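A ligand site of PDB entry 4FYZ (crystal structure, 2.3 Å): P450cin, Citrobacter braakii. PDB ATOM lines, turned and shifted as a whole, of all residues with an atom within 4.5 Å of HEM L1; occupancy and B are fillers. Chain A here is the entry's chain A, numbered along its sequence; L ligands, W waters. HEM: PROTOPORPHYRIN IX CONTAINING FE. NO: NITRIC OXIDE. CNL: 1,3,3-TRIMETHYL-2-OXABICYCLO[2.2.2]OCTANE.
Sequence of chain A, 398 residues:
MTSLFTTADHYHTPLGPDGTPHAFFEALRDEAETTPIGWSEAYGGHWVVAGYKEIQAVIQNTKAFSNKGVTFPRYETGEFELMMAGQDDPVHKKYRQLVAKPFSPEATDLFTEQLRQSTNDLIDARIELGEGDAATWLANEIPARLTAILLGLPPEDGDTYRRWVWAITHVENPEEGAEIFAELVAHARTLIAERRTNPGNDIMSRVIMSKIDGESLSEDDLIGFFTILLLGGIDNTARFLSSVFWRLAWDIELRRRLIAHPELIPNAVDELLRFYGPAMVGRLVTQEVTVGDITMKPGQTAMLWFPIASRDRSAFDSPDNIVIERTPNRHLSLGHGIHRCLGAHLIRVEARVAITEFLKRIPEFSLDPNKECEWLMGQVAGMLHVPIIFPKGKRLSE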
ATOM      1  N   ILE A  59      38.084  27.525 -17.017  1.00  0.00           N
ATOM      2  CA  ILE A  59      36.765  26.941 -16.834  1.00  0.00           C
ATOM      3  C   ILE A  59      36.066  26.638 -18.167  1.00  0.00           C
ATOM      4  O   ILE A  59      35.218  25.752 -18.240  1.00  0.00           O
ATOM      5  CB  ILE A  59      35.922  27.848 -15.904  1.00  0.00           C
ATOM      6  CG1 ILE A  59      35.377  27.029 -14.729  1.00  0.00           C
ATOM      7  CG2 ILE A  59      34.835  28.569 -16.670  1.00  0.00           C
ATOM      8  CD1 ILE A  59      34.601  27.867 -13.723  1.00  0.00           C
ATOM      9  N   ASN A  67      37.001  17.873 -14.158  1.00  0.00           N
ATOM     10  CA  ASN A  67      36.282  18.045 -12.897  1.00  0.00           C
ATOM     11  C   ASN A  67      36.461  16.900 -11.914  1.00  0.00           C
ATOM     12  O   ASN A  67      35.832  16.883 -10.849  1.00  0.00           O
ATOM     13  CB  ASN A  67      34.810  18.339 -13.149  1.00  0.00           C
ATOM     14  CG  ASN A  67      34.509  19.810 -13.124  1.00  0.00           C
ATOM     15  OD1 ASN A  67      35.060  20.576 -13.922  1.00  0.00           O
ATOM     16  ND2 ASN A  67      33.673  20.236 -12.193  1.00  0.00           N
ATOM     17  N   VAL A  70      37.545  18.435  -8.871  1.00  0.00           N
ATOM     18  CA  VAL A  70      36.661  19.510  -8.415  1.00  0.00           C
ATOM     19  C   VAL A  70      36.822  19.854  -6.923  1.00  0.00           C
ATOM     20  O   VAL A  70      36.707  21.020  -6.544  1.00  0.00           O
ATOM     21  CB  VAL A  70      35.157  19.208  -8.748  1.00  0.00           C
ATOM     22  CG1 VAL A  70      34.597  18.073  -7.863  1.00  0.00           C
ATOM     23  CG2 VAL A  70      34.306  20.464  -8.628  1.00  0.00           C
ATOM     24  N   MET A  84      27.524  14.911 -11.234  1.00  0.00           N
ATOM     25  CA  MET A  84      27.614  16.125 -12.028  1.00  0.00           C
ATOM     26  C   MET A  84      28.934  16.852 -11.760  1.00  0.00           C
ATOM     27  O   MET A  84      29.763  16.959 -12.660  1.00  0.00           O
ATOM     28  CB  MET A  84      26.383  17.016 -11.841  1.00  0.00           C
ATOM     29  CG  MET A  84      25.086  16.311 -12.250  1.00  0.00           C
ATOM     30  SD  MET A  84      23.613  17.142 -11.665  1.00  0.00           S
ATOM     31  CE  MET A  84      23.635  16.690  -9.931  1.00  0.00           C
ATOM     32  N   ALA A  85      29.147  17.311 -10.520  1.00  0.00           N
ATOM     33  CA  ALA A  85      30.289  18.172 -10.199  1.00  0.00           C
ATOM     34  C   ALA A  85      31.639  17.497 -10.377  1.00  0.00           C
ATOM     35  O   ALA A  85      32.609  18.146 -10.745  1.00  0.00           O
ATOM     36  CB  ALA A  85      30.155  18.714  -8.784  1.00  0.00           C
ATOM     37  N   HIS A  92      28.874  13.573 -17.578  1.00  0.00           N
ATOM     38  CA  HIS A  92      28.320  14.699 -16.805  1.00  0.00           C
ATOM     39  C   HIS A  92      26.976  15.204 -17.346  1.00  0.00           C
ATOM     40  O   HIS A  92      26.006  15.287 -16.597  1.00  0.00           O
ATOM     41  CB  HIS A  92      29.335  15.843 -16.732  1.00  0.00           C
ATOM     42  CG  HIS A  92      28.705  17.201 -16.599  1.00  0.00           C
ATOM     43  ND1 HIS A  92      28.431  17.999 -17.690  1.00  0.00           N
ATOM     44  CD2 HIS A  92      28.305  17.900 -15.510  1.00  0.00           C
ATOM     45  CE1 HIS A  92      27.873  19.123 -17.272  1.00  0.00           C
ATOM     46  NE2 HIS A  92      27.789  19.093 -15.958  1.00  0.00           N
ATOM     47  N   ARG A  96      23.146  15.411 -15.497  1.00  0.00           N
ATOM     48  CA  ARG A  96      22.524  16.680 -15.169  1.00  0.00           C
ATOM     49  C   ARG A  96      21.110  16.778 -15.770  1.00  0.00           C
ATOM     50  O   ARG A  96      20.189  17.285 -15.126  1.00  0.00           O
ATOM     51  CB  ARG A  96      23.383  17.862 -15.620  1.00  0.00           C
ATOM     52  CG  ARG A  96      23.104  19.132 -14.864  1.00  0.00           C
ATOM     53  CD  ARG A  96      23.661  20.337 -15.579  1.00  0.00           C
ATOM     54  NE  ARG A  96      22.945  21.557 -15.194  1.00  0.00           N
ATOM     55  CZ  ARG A  96      23.514  22.583 -14.558  1.00  0.00           C
ATOM     56  NH1 ARG A  96      24.794  22.526 -14.236  1.00  0.00           N
ATOM     57  NH2 ARG A  96      22.795  23.660 -14.247  1.00  0.00           N
ATOM     58  N   PHE A 103      15.063  21.402 -11.165  1.00  0.00           N
ATOM     59  CA  PHE A 103      15.824  22.533 -10.657  1.00  0.00           C
ATOM     60  C   PHE A 103      15.656  23.794 -11.515  1.00  0.00           C
ATOM     61  O   PHE A 103      16.311  24.807 -11.274  1.00  0.00           O
ATOM     62  CB  PHE A 103      17.305  22.180 -10.489  1.00  0.00           C
ATOM     63  CG  PHE A 103      17.595  21.455  -9.205  1.00  0.00           C
ATOM     64  CD1 PHE A 103      17.706  22.151  -8.012  1.00  0.00           C
ATOM     65  CD2 PHE A 103      17.721  20.071  -9.184  1.00  0.00           C
ATOM     66  CE1 PHE A 103      17.952  21.487  -6.814  1.00  0.00           C
ATOM     67  CE2 PHE A 103      17.977  19.401  -8.002  1.00  0.00           C
ATOM     68  CZ  PHE A 103      18.090  20.111  -6.813  1.00  0.00           C
ATOM     69  N   LEU A 150      13.758  18.550  -0.515  1.00  0.00           N
ATOM     70  CA  LEU A 150      14.232  18.131  -1.827  1.00  0.00           C
ATOM     71  C   LEU A 150      14.669  16.659  -1.843  1.00  0.00           C
ATOM     72  O   LEU A 150      14.497  15.968  -2.843  1.00  0.00           O
ATOM     73  CB  LEU A 150      15.391  19.008  -2.270  1.00  0.00           C
ATOM     74  CG  LEU A 150      15.111  20.476  -2.585  1.00  0.00           C
ATOM     75  CD1 LEU A 150      16.416  21.208  -2.938  1.00  0.00           C
ATOM     76  CD2 LEU A 150      14.069  20.605  -3.703  1.00  0.00           C
ATOM     77  N   ILE A 228      25.951  15.306  -3.207  1.00  0.00           N
ATOM     78  CA  ILE A 228      26.237  16.666  -3.665  1.00  0.00           C
ATOM     79  C   ILE A 228      25.090  17.628  -3.366  1.00  0.00           C
ATOM     80  O   ILE A 228      25.323  18.757  -2.934  1.00  0.00           O
ATOM     81  CB  ILE A 228      26.684  16.745  -5.142  1.00  0.00           C
ATOM     82  CG1 ILE A 228      26.870  18.207  -5.526  1.00  0.00           C
ATOM     83  CG2 ILE A 228      25.700  16.040  -6.057  1.00  0.00           C
ATOM     84  CD1 ILE A 228      27.296  18.405  -6.923  1.00  0.00           C
ATOM     85  N   LEU A 229      23.854  17.159  -3.539  1.00  0.00           N
ATOM     86  CA  LEU A 229      22.694  17.989  -3.215  1.00  0.00           C
ATOM     87  C   LEU A 229      22.702  18.370  -1.743  1.00  0.00           C
ATOM     88  O   LEU A 229      22.471  19.522  -1.393  1.00  0.00           O
ATOM     89  CB  LEU A 229      21.379  17.317  -3.621  1.00  0.00           C
ATOM     90  CG  LEU A 229      21.255  17.044  -5.128  1.00  0.00           C
ATOM     91  CD1 LEU A 229      19.856  16.564  -5.506  1.00  0.00           C
ATOM     92  CD2 LEU A 229      21.637  18.270  -5.921  1.00  0.00           C
ATOM     93  N   GLY A 232      25.406  21.125  -1.339  1.00  0.00           N
ATOM     94  CA  GLY A 232      24.953  22.414  -1.831  1.00  0.00           C
ATOM     95  C   GLY A 232      24.121  23.205  -0.817  1.00  0.00           C
ATOM     96  O   GLY A 232      24.262  24.421  -0.715  1.00  0.00           O
ATOM     97  N   GLY A 233      23.287  22.506  -0.055  1.00  0.00           N
ATOM     98  CA  GLY A 233      22.438  23.155   0.937  1.00  0.00           C
ATOM     99  C   GLY A 233      23.122  23.414   2.264  1.00  0.00           C
ATOM    100  O   GLY A 233      23.273  24.574   2.697  1.00  0.00           O
ATOM    101  N   ASN A 236      27.393  25.053   1.323  1.00  0.00           N
ATOM    102  CA  ASN A 236      27.479  26.273   0.523  1.00  0.00           C
ATOM    103  C   ASN A 236      26.479  27.375   0.875  1.00  0.00           C
ATOM    104  O   ASN A 236      26.882  28.520   1.100  1.00  0.00           O
ATOM    105  CB  ASN A 236      27.369  25.949  -0.969  1.00  0.00           C
ATOM    106  CG  ASN A 236      28.291  24.822  -1.396  1.00  0.00           C
ATOM    107  OD1 ASN A 236      28.756  24.033  -0.558  1.00  0.00           O
ATOM    108  ND2 ASN A 236      28.569  24.753  -2.693  1.00  0.00           N
ATOM    109  N   THR A 237      25.187  27.050   0.923  1.00  0.00           N
ATOM    110  CA  THR A 237      24.151  28.050   1.191  1.00  0.00           C
ATOM    111  C   THR A 237      24.197  28.541   2.622  1.00  0.00           C
ATOM    112  O   THR A 237      24.083  29.744   2.880  1.00  0.00           O
ATOM    113  CB  THR A 237      22.717  27.556   0.881  1.00  0.00           C
ATOM    114  OG1 THR A 237      22.652  27.005  -0.443  1.00  0.00           O
ATOM    115  CG2 THR A 237      21.743  28.700   0.965  1.00  0.00           C
ATOM    116  N   PHE A 240      27.092  30.952   3.006  1.00  0.00           N
ATOM    117  CA  PHE A 240      26.798  32.194   2.310  1.00  0.00           C
ATOM    118  C   PHE A 240      25.818  33.035   3.107  1.00  0.00           C
ATOM    119  O   PHE A 240      26.071  34.215   3.363  1.00  0.00           O
ATOM    120  CB  PHE A 240      26.216  31.935   0.911  1.00  0.00           C
ATOM    121  CG  PHE A 240      25.661  33.156   0.271  1.00  0.00           C
ATOM    122  CD1 PHE A 240      24.299  33.288   0.044  1.00  0.00           C
ATOM    123  CD2 PHE A 240      26.493  34.229  -0.037  1.00  0.00           C
ATOM    124  CE1 PHE A 240      23.780  34.436  -0.537  1.00  0.00           C
ATOM    125  CE2 PHE A 240      25.983  35.397  -0.618  1.00  0.00           C
ATOM    126  CZ  PHE A 240      24.622  35.503  -0.860  1.00  0.00           C
ATOM    127  N   LEU A 273      26.352  37.813  -3.421  1.00  0.00           N
ATOM    128  CA  LEU A 273      26.962  36.601  -3.983  1.00  0.00           C
ATOM    129  C   LEU A 273      28.362  36.867  -4.543  1.00  0.00           C
ATOM    130  O   LEU A 273      29.288  36.075  -4.327  1.00  0.00           O
ATOM    131  CB  LEU A 273      26.084  35.998  -5.100  1.00  0.00           C
ATOM    132  CG  LEU A 273      24.883  35.158  -4.720  1.00  0.00           C
ATOM    133  CD1 LEU A 273      24.039  34.791  -5.972  1.00  0.00           C
ATOM    134  CD2 LEU A 273      25.329  33.901  -3.975  1.00  0.00           C
ATOM    135  N   PRO A 278      31.077  31.928  -1.162  1.00  0.00           N
ATOM    136  CA  PRO A 278      31.949  31.089  -0.340  1.00  0.00           C
ATOM    137  C   PRO A 278      32.835  30.096  -1.104  1.00  0.00           C
ATOM    138  O   PRO A 278      33.839  29.657  -0.548  1.00  0.00           O
ATOM    139  CB  PRO A 278      30.952  30.285   0.506  1.00  0.00           C
ATOM    140  CG  PRO A 278      29.740  30.202  -0.324  1.00  0.00           C
ATOM    141  CD  PRO A 278      29.665  31.519  -1.060  1.00  0.00           C
ATOM    142  N   ALA A 279      32.477  29.767  -2.343  1.00  0.00           N
ATOM    143  CA  ALA A 279      33.096  28.625  -3.009  1.00  0.00           C
ATOM    144  C   ALA A 279      34.359  28.935  -3.803  1.00  0.00           C
ATOM    145  O   ALA A 279      34.545  30.032  -4.328  1.00  0.00           O
ATOM    146  CB  ALA A 279      32.059  27.912  -3.905  1.00  0.00           C
ATOM    147  N   VAL A 281      36.741  26.150  -6.550  1.00  0.00           N
ATOM    148  CA  VAL A 281      36.702  24.801  -7.106  1.00  0.00           C
ATOM    149  C   VAL A 281      38.083  24.459  -7.661  1.00  0.00           C
ATOM    150  O   VAL A 281      38.866  25.350  -7.995  1.00  0.00           O
ATOM    151  CB  VAL A 281      35.648  24.660  -8.247  1.00  0.00           C
ATOM    152  CG1 VAL A 281      34.264  25.132  -7.800  1.00  0.00           C
ATOM    153  CG2 VAL A 281      36.074  25.425  -9.462  1.00  0.00           C
ATOM    154  N   ARG A 283      40.543  22.029 -10.497  1.00  0.00           N
ATOM    155  CA  ARG A 283      40.545  21.367 -11.803  1.00  0.00           C
ATOM    156  C   ARG A 283      41.767  20.465 -11.882  1.00  0.00           C
ATOM    157  O   ARG A 283      42.871  20.880 -11.514  1.00  0.00           O
ATOM    158  CB  ARG A 283      40.583  22.384 -12.940  1.00  0.00           C
ATOM    159  CG  ARG A 283      39.295  23.210 -13.107  1.00  0.00           C
ATOM    160  CD  ARG A 283      38.132  22.316 -13.490  1.00  0.00           C
ATOM    161  NE  ARG A 283      36.925  23.036 -13.889  1.00  0.00           N
ATOM    162  CZ  ARG A 283      35.910  23.328 -13.069  1.00  0.00           C
ATOM    163  NH1 ARG A 283      35.949  22.974 -11.786  1.00  0.00           N
ATOM    164  NH2 ARG A 283      34.847  23.959 -13.544  1.00  0.00           N
ATOM    165  N   PHE A 306      37.742  31.882  -7.094  1.00  0.00           N
ATOM    166  CA  PHE A 306      36.614  32.751  -7.422  1.00  0.00           C
ATOM    167  C   PHE A 306      36.553  34.115  -6.664  1.00  0.00           C
ATOM    168  O   PHE A 306      36.369  35.156  -7.309  1.00  0.00           O
ATOM    169  CB  PHE A 306      35.271  31.997  -7.292  1.00  0.00           C
ATOM    170  CG  PHE A 306      35.063  30.918  -8.338  1.00  0.00           C
ATOM    171  CD1 PHE A 306      34.285  29.793  -8.053  1.00  0.00           C
ATOM    172  CD2 PHE A 306      35.627  31.010  -9.602  1.00  0.00           C
ATOM    173  CE1 PHE A 306      34.082  28.786  -9.010  1.00  0.00           C
ATOM    174  CE2 PHE A 306      35.403  30.013 -10.563  1.00  0.00           C
ATOM    175  CZ  PHE A 306      34.639  28.897 -10.261  1.00  0.00           C
ATOM    176  N   LEU A 332      31.664  35.059 -10.600  1.00  0.00           N
ATOM    177  CA  LEU A 332      31.848  33.635 -10.798  1.00  0.00           C
ATOM    178  C   LEU A 332      31.412  32.820  -9.583  1.00  0.00           C
ATOM    179  O   LEU A 332      31.663  31.617  -9.512  1.00  0.00           O
ATOM    180  CB  LEU A 332      33.325  33.338 -11.115  1.00  0.00           C
ATOM    181  CG  LEU A 332      33.836  33.922 -12.437  1.00  0.00           C
ATOM    182  CD1 LEU A 332      35.346  33.814 -12.555  1.00  0.00           C
ATOM    183  CD2 LEU A 332      33.193  33.212 -13.605  1.00  0.00           C
ATOM    184  N   SER A 333      30.769  33.477  -8.615  1.00  0.00           N
ATOM    185  CA  SER A 333      30.345  32.812  -7.384  1.00  0.00           C
ATOM    186  C   SER A 333      29.480  31.534  -7.599  1.00  0.00           C
ATOM    187  O   SER A 333      29.491  30.622  -6.762  1.00  0.00           O
ATOM    188  CB  SER A 333      29.636  33.802  -6.463  1.00  0.00           C
ATOM    189  OG  SER A 333      30.536  34.813  -6.011  1.00  0.00           O
ATOM    190  N   LEU A 334      28.749  31.468  -8.705  1.00  0.00           N
ATOM    191  CA  LEU A 334      27.970  30.262  -9.015  1.00  0.00           C
ATOM    192  C   LEU A 334      28.560  29.466 -10.174  1.00  0.00           C
ATOM    193  O   LEU A 334      27.884  28.646 -10.800  1.00  0.00           O
ATOM    194  CB  LEU A 334      26.498  30.598  -9.306  1.00  0.00           C
ATOM    195  CG  LEU A 334      25.726  31.175  -8.121  1.00  0.00           C
ATOM    196  CD1 LEU A 334      24.307  31.535  -8.523  1.00  0.00           C
ATOM    197  CD2 LEU A 334      25.761  30.189  -6.951  1.00  0.00           C
ATOM    198  N   GLY A 335      29.836  29.702 -10.457  1.00  0.00           N
ATOM    199  CA  GLY A 335      30.493  29.061 -11.568  1.00  0.00           C
ATOM    200  C   GLY A 335      30.079  29.649 -12.904  1.00  0.00           C
ATOM    201  O   GLY A 335      29.319  30.623 -12.972  1.00  0.00           O
ATOM    202  N   ILE A 338      29.632  24.733 -18.241  1.00  0.00           N
ATOM    203  CA  ILE A 338      28.828  23.520 -18.161  1.00  0.00           C
ATOM    204  C   ILE A 338      28.610  23.019 -16.728  1.00  0.00           C
ATOM    205  O   ILE A 338      27.721  22.210 -16.474  1.00  0.00           O
ATOM    206  CB  ILE A 338      29.458  22.378 -19.005  1.00  0.00           C
ATOM    207  CG1 ILE A 338      30.799  21.963 -18.399  1.00  0.00           C
ATOM    208  CG2 ILE A 338      29.648  22.796 -20.463  1.00  0.00           C
ATOM    209  CD1 ILE A 338      31.391  20.701 -19.029  1.00  0.00           C
ATOM    210  N   HIS A 339      29.425  23.489 -15.785  1.00  0.00           N
ATOM    211  CA  HIS A 339      29.241  23.085 -14.389  1.00  0.00           C
ATOM    212  C   HIS A 339      28.546  24.129 -13.539  1.00  0.00           C
ATOM    213  O   HIS A 339      28.489  23.988 -12.304  1.00  0.00           O
ATOM    214  CB  HIS A 339      30.567  22.708 -13.757  1.00  0.00           C
ATOM    215  CG  HIS A 339      31.138  21.445 -14.313  1.00  0.00           C
ATOM    216  ND1 HIS A 339      30.608  20.204 -14.045  1.00  0.00           N
ATOM    217  CD2 HIS A 339      32.168  21.238 -15.166  1.00  0.00           C
ATOM    218  CE1 HIS A 339      31.302  19.286 -14.671  1.00  0.00           C
ATOM    219  NE2 HIS A 339      32.261  19.884 -15.359  1.00  0.00           N
ATOM    220  N   ARG A 340      28.037  25.168 -14.198  1.00  0.00           N
ATOM    221  CA  ARG A 340      27.299  26.252 -13.559  1.00  0.00           C
ATOM    222  C   ARG A 340      26.325  25.710 -12.521  1.00  0.00           C
ATOM    223  O   ARG A 340      25.626  24.717 -12.772  1.00  0.00           O
ATOM    224  CB  ARG A 340      26.566  27.075 -14.620  1.00  0.00           C
ATOM    225  CG  ARG A 340      25.044  27.176 -14.445  1.00  0.00           C
ATOM    226  CD  ARG A 340      24.273  27.044 -15.771  1.00  0.00           C
ATOM    227  NE  ARG A 340      24.060  25.648 -16.159  1.00  0.00           N
ATOM    228  CZ  ARG A 340      24.353  25.149 -17.358  1.00  0.00           C
ATOM    229  NH1 ARG A 340      24.879  25.914 -18.306  1.00  0.00           N
ATOM    230  NH2 ARG A 340      24.109  23.866 -17.609  1.00  0.00           N
ATOM    231  N   CYS A 341      26.314  26.330 -11.339  1.00  0.00           N
ATOM    232  CA  CYS A 341      25.490  25.903 -10.227  1.00  0.00           C
ATOM    233  C   CYS A 341      24.045  25.520 -10.606  1.00  0.00           C
ATOM    234  O   CYS A 341      23.314  26.290 -11.232  1.00  0.00           O
ATOM    235  CB  CYS A 341      25.479  26.962  -9.124  1.00  0.00           C
ATOM    236  SG  CYS A 341      24.633  26.431  -7.622  1.00  0.00           S
ATOM    237  N   LEU A 342      23.665  24.305 -10.231  1.00  0.00           N
ATOM    238  CA  LEU A 342      22.348  23.737 -10.479  1.00  0.00           C
ATOM    239  C   LEU A 342      21.293  24.453  -9.648  1.00  0.00           C
ATOM    240  O   LEU A 342      20.205  24.777 -10.129  1.00  0.00           O
ATOM    241  CB  LEU A 342      22.370  22.254 -10.084  1.00  0.00           C
ATOM    242  CG  LEU A 342      21.621  21.141 -10.824  1.00  0.00           C
ATOM    243  CD1 LEU A 342      21.049  20.158  -9.804  1.00  0.00           C
ATOM    244  CD2 LEU A 342      20.556  21.657 -11.786  1.00  0.00           C
ATOM    245  N   GLY A 343      21.618  24.720  -8.384  1.00  0.00           N
ATOM    246  CA  GLY A 343      20.703  25.454  -7.523  1.00  0.00           C
ATOM    247  C   GLY A 343      20.355  26.901  -7.920  1.00  0.00           C
ATOM    248  O   GLY A 343      19.383  27.445  -7.407  1.00  0.00           O
ATOM    249  N   ILE A 347      18.695  29.285  -5.181  1.00  0.00           N
ATOM    250  CA  ILE A 347      19.453  29.952  -4.134  1.00  0.00           C
ATOM    251  C   ILE A 347      19.182  31.480  -4.098  1.00  0.00           C
ATOM    252  O   ILE A 347      19.032  32.043  -3.018  1.00  0.00           O
ATOM    253  CB  ILE A 347      20.977  29.527  -4.025  1.00  0.00           C
ATOM    254  CG1 ILE A 347      21.922  30.714  -4.132  1.00  0.00           C
ATOM    255  CG2 ILE A 347      21.345  28.439  -5.034  1.00  0.00           C
ATOM    256  CD1 ILE A 347      22.225  31.100  -5.547  1.00  0.00           C
HETATM  257  CHA HEM L   1      28.088  23.572  -9.057  1.00  0.00           C
HETATM  258  CHB HEM L   1      28.509  27.289  -5.858  1.00  0.00           C
HETATM  259  CHC HEM L   1      24.223  26.037  -3.755  1.00  0.00           C
HETATM  260  CHD HEM L   1      24.036  22.056  -6.610  1.00  0.00           C
HETATM  261  C1A HEM L   1      28.583  24.737  -8.454  1.00  0.00           C
HETATM  262  C2A HEM L   1      29.704  25.565  -8.854  1.00  0.00           C
HETATM  263  C3A HEM L   1      29.818  26.582  -7.954  1.00  0.00           C
HETATM  264  C4A HEM L   1      28.761  26.467  -6.957  1.00  0.00           C
HETATM  265  CMA HEM L   1      30.873  27.711  -7.974  1.00  0.00           C
HETATM  266  CAA HEM L   1      30.636  25.327 -10.073  1.00  0.00           C
HETATM  267  CBA HEM L   1      31.346  23.980  -9.905  1.00  0.00           C
HETATM  268  CGA HEM L   1      32.509  23.843 -10.860  1.00  0.00           C
HETATM  269  O1A HEM L   1      32.776  24.760 -11.675  1.00  0.00           O
HETATM  270  O2A HEM L   1      33.189  22.789 -10.787  1.00  0.00           O
HETATM  271  C1B HEM L   1      27.385  27.346  -5.023  1.00  0.00           C
HETATM  272  C2B HEM L   1      27.048  28.363  -4.043  1.00  0.00           C
HETATM  273  C3B HEM L   1      25.869  28.011  -3.453  1.00  0.00           C
HETATM  274  C4B HEM L   1      25.388  26.765  -4.044  1.00  0.00           C
HETATM  275  CMB HEM L   1      27.944  29.604  -3.772  1.00  0.00           C
HETATM  276  CAB HEM L   1      25.059  28.751  -2.359  1.00  0.00           C
HETATM  277  CBB HEM L   1      25.253  30.037  -2.042  1.00  0.00           C
HETATM  278  C1C HEM L   1      23.745  24.861  -4.332  1.00  0.00           C
HETATM  279  C2C HEM L   1      22.511  24.125  -4.069  1.00  0.00           C
HETATM  280  C3C HEM L   1      22.469  23.028  -4.873  1.00  0.00           C
HETATM  281  C4C HEM L   1      23.673  23.008  -5.672  1.00  0.00           C
HETATM  282  CMC HEM L   1      21.469  24.591  -3.033  1.00  0.00           C
HETATM  283  CAC HEM L   1      21.428  21.889  -5.011  1.00  0.00           C
HETATM  284  CBC HEM L   1      20.429  21.673  -4.140  1.00  0.00           C
HETATM  285  C1D HEM L   1      25.096  22.046  -7.513  1.00  0.00           C
HETATM  286  C2D HEM L   1      25.396  21.018  -8.475  1.00  0.00           C
HETATM  287  C3D HEM L   1      26.653  21.477  -9.237  1.00  0.00           C
HETATM  288  C4D HEM L   1      27.016  22.759  -8.682  1.00  0.00           C
HETATM  289  CMD HEM L   1      24.610  19.726  -8.685  1.00  0.00           C
HETATM  290  CAD HEM L   1      27.340  20.720 -10.376  1.00  0.00           C
HETATM  291  CBD HEM L   1      26.517  21.060 -11.617  1.00  0.00           C
HETATM  292  CGD HEM L   1      27.200  20.481 -12.819  1.00  0.00           C
HETATM  293  O1D HEM L   1      26.663  20.667 -13.955  1.00  0.00           O
HETATM  294  O2D HEM L   1      28.279  19.847 -12.626  1.00  0.00           O
HETATM  295  NA  HEM L   1      28.076  25.327  -7.319  1.00  0.00           N
HETATM  296  NB  HEM L   1      26.363  26.438  -4.950  1.00  0.00           N
HETATM  297  NC  HEM L   1      24.373  24.131  -5.308  1.00  0.00           N
HETATM  298  ND  HEM L   1      26.071  23.015  -7.709  1.00  0.00           N
HETATM  299 FE   HEM L   1      26.351  24.665  -6.220  1.00  0.00          FE
HETATM  300  N    NO L   2      27.150  23.530  -5.083  1.00  0.00           N
HETATM  301  O    NO L   2      26.896  22.496  -4.658  1.00  0.00           O
HETATM  302  C1  CNL L   3      30.216  21.271  -4.179  1.00  0.00           C
HETATM  303  C2  CNL L   3      29.949  21.280  -5.639  1.00  0.00           C
HETATM  304  C3  CNL L   3      31.062  21.873  -6.414  1.00  0.00           C
HETATM  305  C4  CNL L   3      32.172  22.369  -5.570  1.00  0.00           C
HETATM  306  C5  CNL L   3      32.641  21.325  -4.714  1.00  0.00           C
HETATM  307  C6  CNL L   3      31.571  20.698  -3.889  1.00  0.00           C
HETATM  308  C7  CNL L   3      29.130  20.631  -3.396  1.00  0.00           C
HETATM  309  C8  CNL L   3      31.536  23.398  -4.642  1.00  0.00           C
HETATM  310  C9  CNL L   3      31.020  24.553  -5.443  1.00  0.00           C
HETATM  311  C10 CNL L   3      32.491  24.002  -3.649  1.00  0.00           C
HETATM  312  O   CNL L   3      30.307  22.705  -3.915  1.00  0.00           O
HETATM  313  O   HOH W   1      30.781  31.067  -4.266  1.00  0.00           O
HETATM  314  O   HOH W   2      19.760  25.813  -0.407  1.00  0.00           O
HETATM  315  O   HOH W   3      31.108  26.374 -13.434  1.00  0.00           O
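A nitrogen (N) of NO L2 binds an iron atom (FE) of HEM L1 (1.8 Å).
The guanidinium group (NH1) of Arg 96 is in salt-bridge range of an oxygen (O1D) of HEM L1 (2.7 Å).
O2D of HEM L1 is in hydrogen-bond range of ND1 of His 339, at 2.8 Å.
NE2 of His 92 sits at hydrogen-bond distance from O1D of HEM L1 (2.8 Å).
An oxygen (O1A) of HEM L1 lies within salt-bridge range of the guanidinium group (NH2) of Arg 283 (2.9 Å).
The side-chain amide nitrogen of Asn 67 lies within hydrogen-bond range of an oxygen (O2A) of HEM L1, 3.0 Å away.
The backbone NH (N) of Ala 85 sits at hydrogen-bond distance from an oxygen (O2D) of HEM L1 (3.4 Å).
ND2 of Asn 236 sits at hydrogen-bond distance from O of NO L2 (3.4 Å).
ND2 of Asn 236 lies within hydrogen-bond range of O of CNL L3, at 3.0 Å.
O of Met 84 lies close to O2D of HEM L1 (3.2 Å).
O of Ile 338 lies close to O1D of HEM L1 (3.1 Å).
SG of Cys 341 sits close to NB of HEM L1.
Residues that only touch HEM L1: Val 70, Phe 103, Ile 228, Leu 229, Gly 232, Asn 236, Thr 237, Phe 240, Pro 278, Val 281, Phe 306, Ser 333, Leu 334, Gly 335, Arg 340, Leu 342, Gly 343 and Ile 347.
Within 4 Å of HEM L1: Asn 67, Val 70, Met 84, Ala 85, His 92, Arg 96, Phe 103, Ile 228, Leu 229, Gly 232, Asn 236, Thr 237, Phe 240, Pro 278, Val 281, Arg 283, Phe 306, Ser 333, Leu 334, Gly 335, Ile 338, His 339, Arg 340, Cys 341, Leu 342, Gly 343 and Ile 347.
The nearest printed residue that does not touch HEM L1 is Gly 233 (4.1 Å).
O of Arg 340 lies within hydrogen-bond range of NH1 of Arg 96, 2.8 Å away.
OD1 of Asn 67 lies close to NE2 of His 339, 3.2 Å away.
O of Ile 338 sits at hydrogen-bond distance from NE2 of His 92.
N of Cys 341 lies within hydrogen-bond range of O of Leu 334, 2.8 Å away.
The backbone NH (N) of Gly 343 lies close to the side-chain sulfur (SG) of Cys 341 (3.5 Å).
The backbone carbonyl oxygen of Ala 85 sits at hydrogen-bond distance from the side-chain amide nitrogen of Asn 67 (2.8 Å).
O of Leu 273 lies within hydrogen-bond range of OG of Ser 333, 2.4 Å away.
The side-chain hydroxyl of Thr 237 lies within hydrogen-bond range of the backbone carbonyl oxygen of Gly 232 (3.1 Å).
Water W3 lies within hydrogen-bond range of an oxygen (O1A) of HEM L1 (2.9 Å) and the backbone NH of Arg 340 (3.4 Å).
Water W1 lies within hydrogen-bond range of O of Ser 333 and N of Ala 279.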
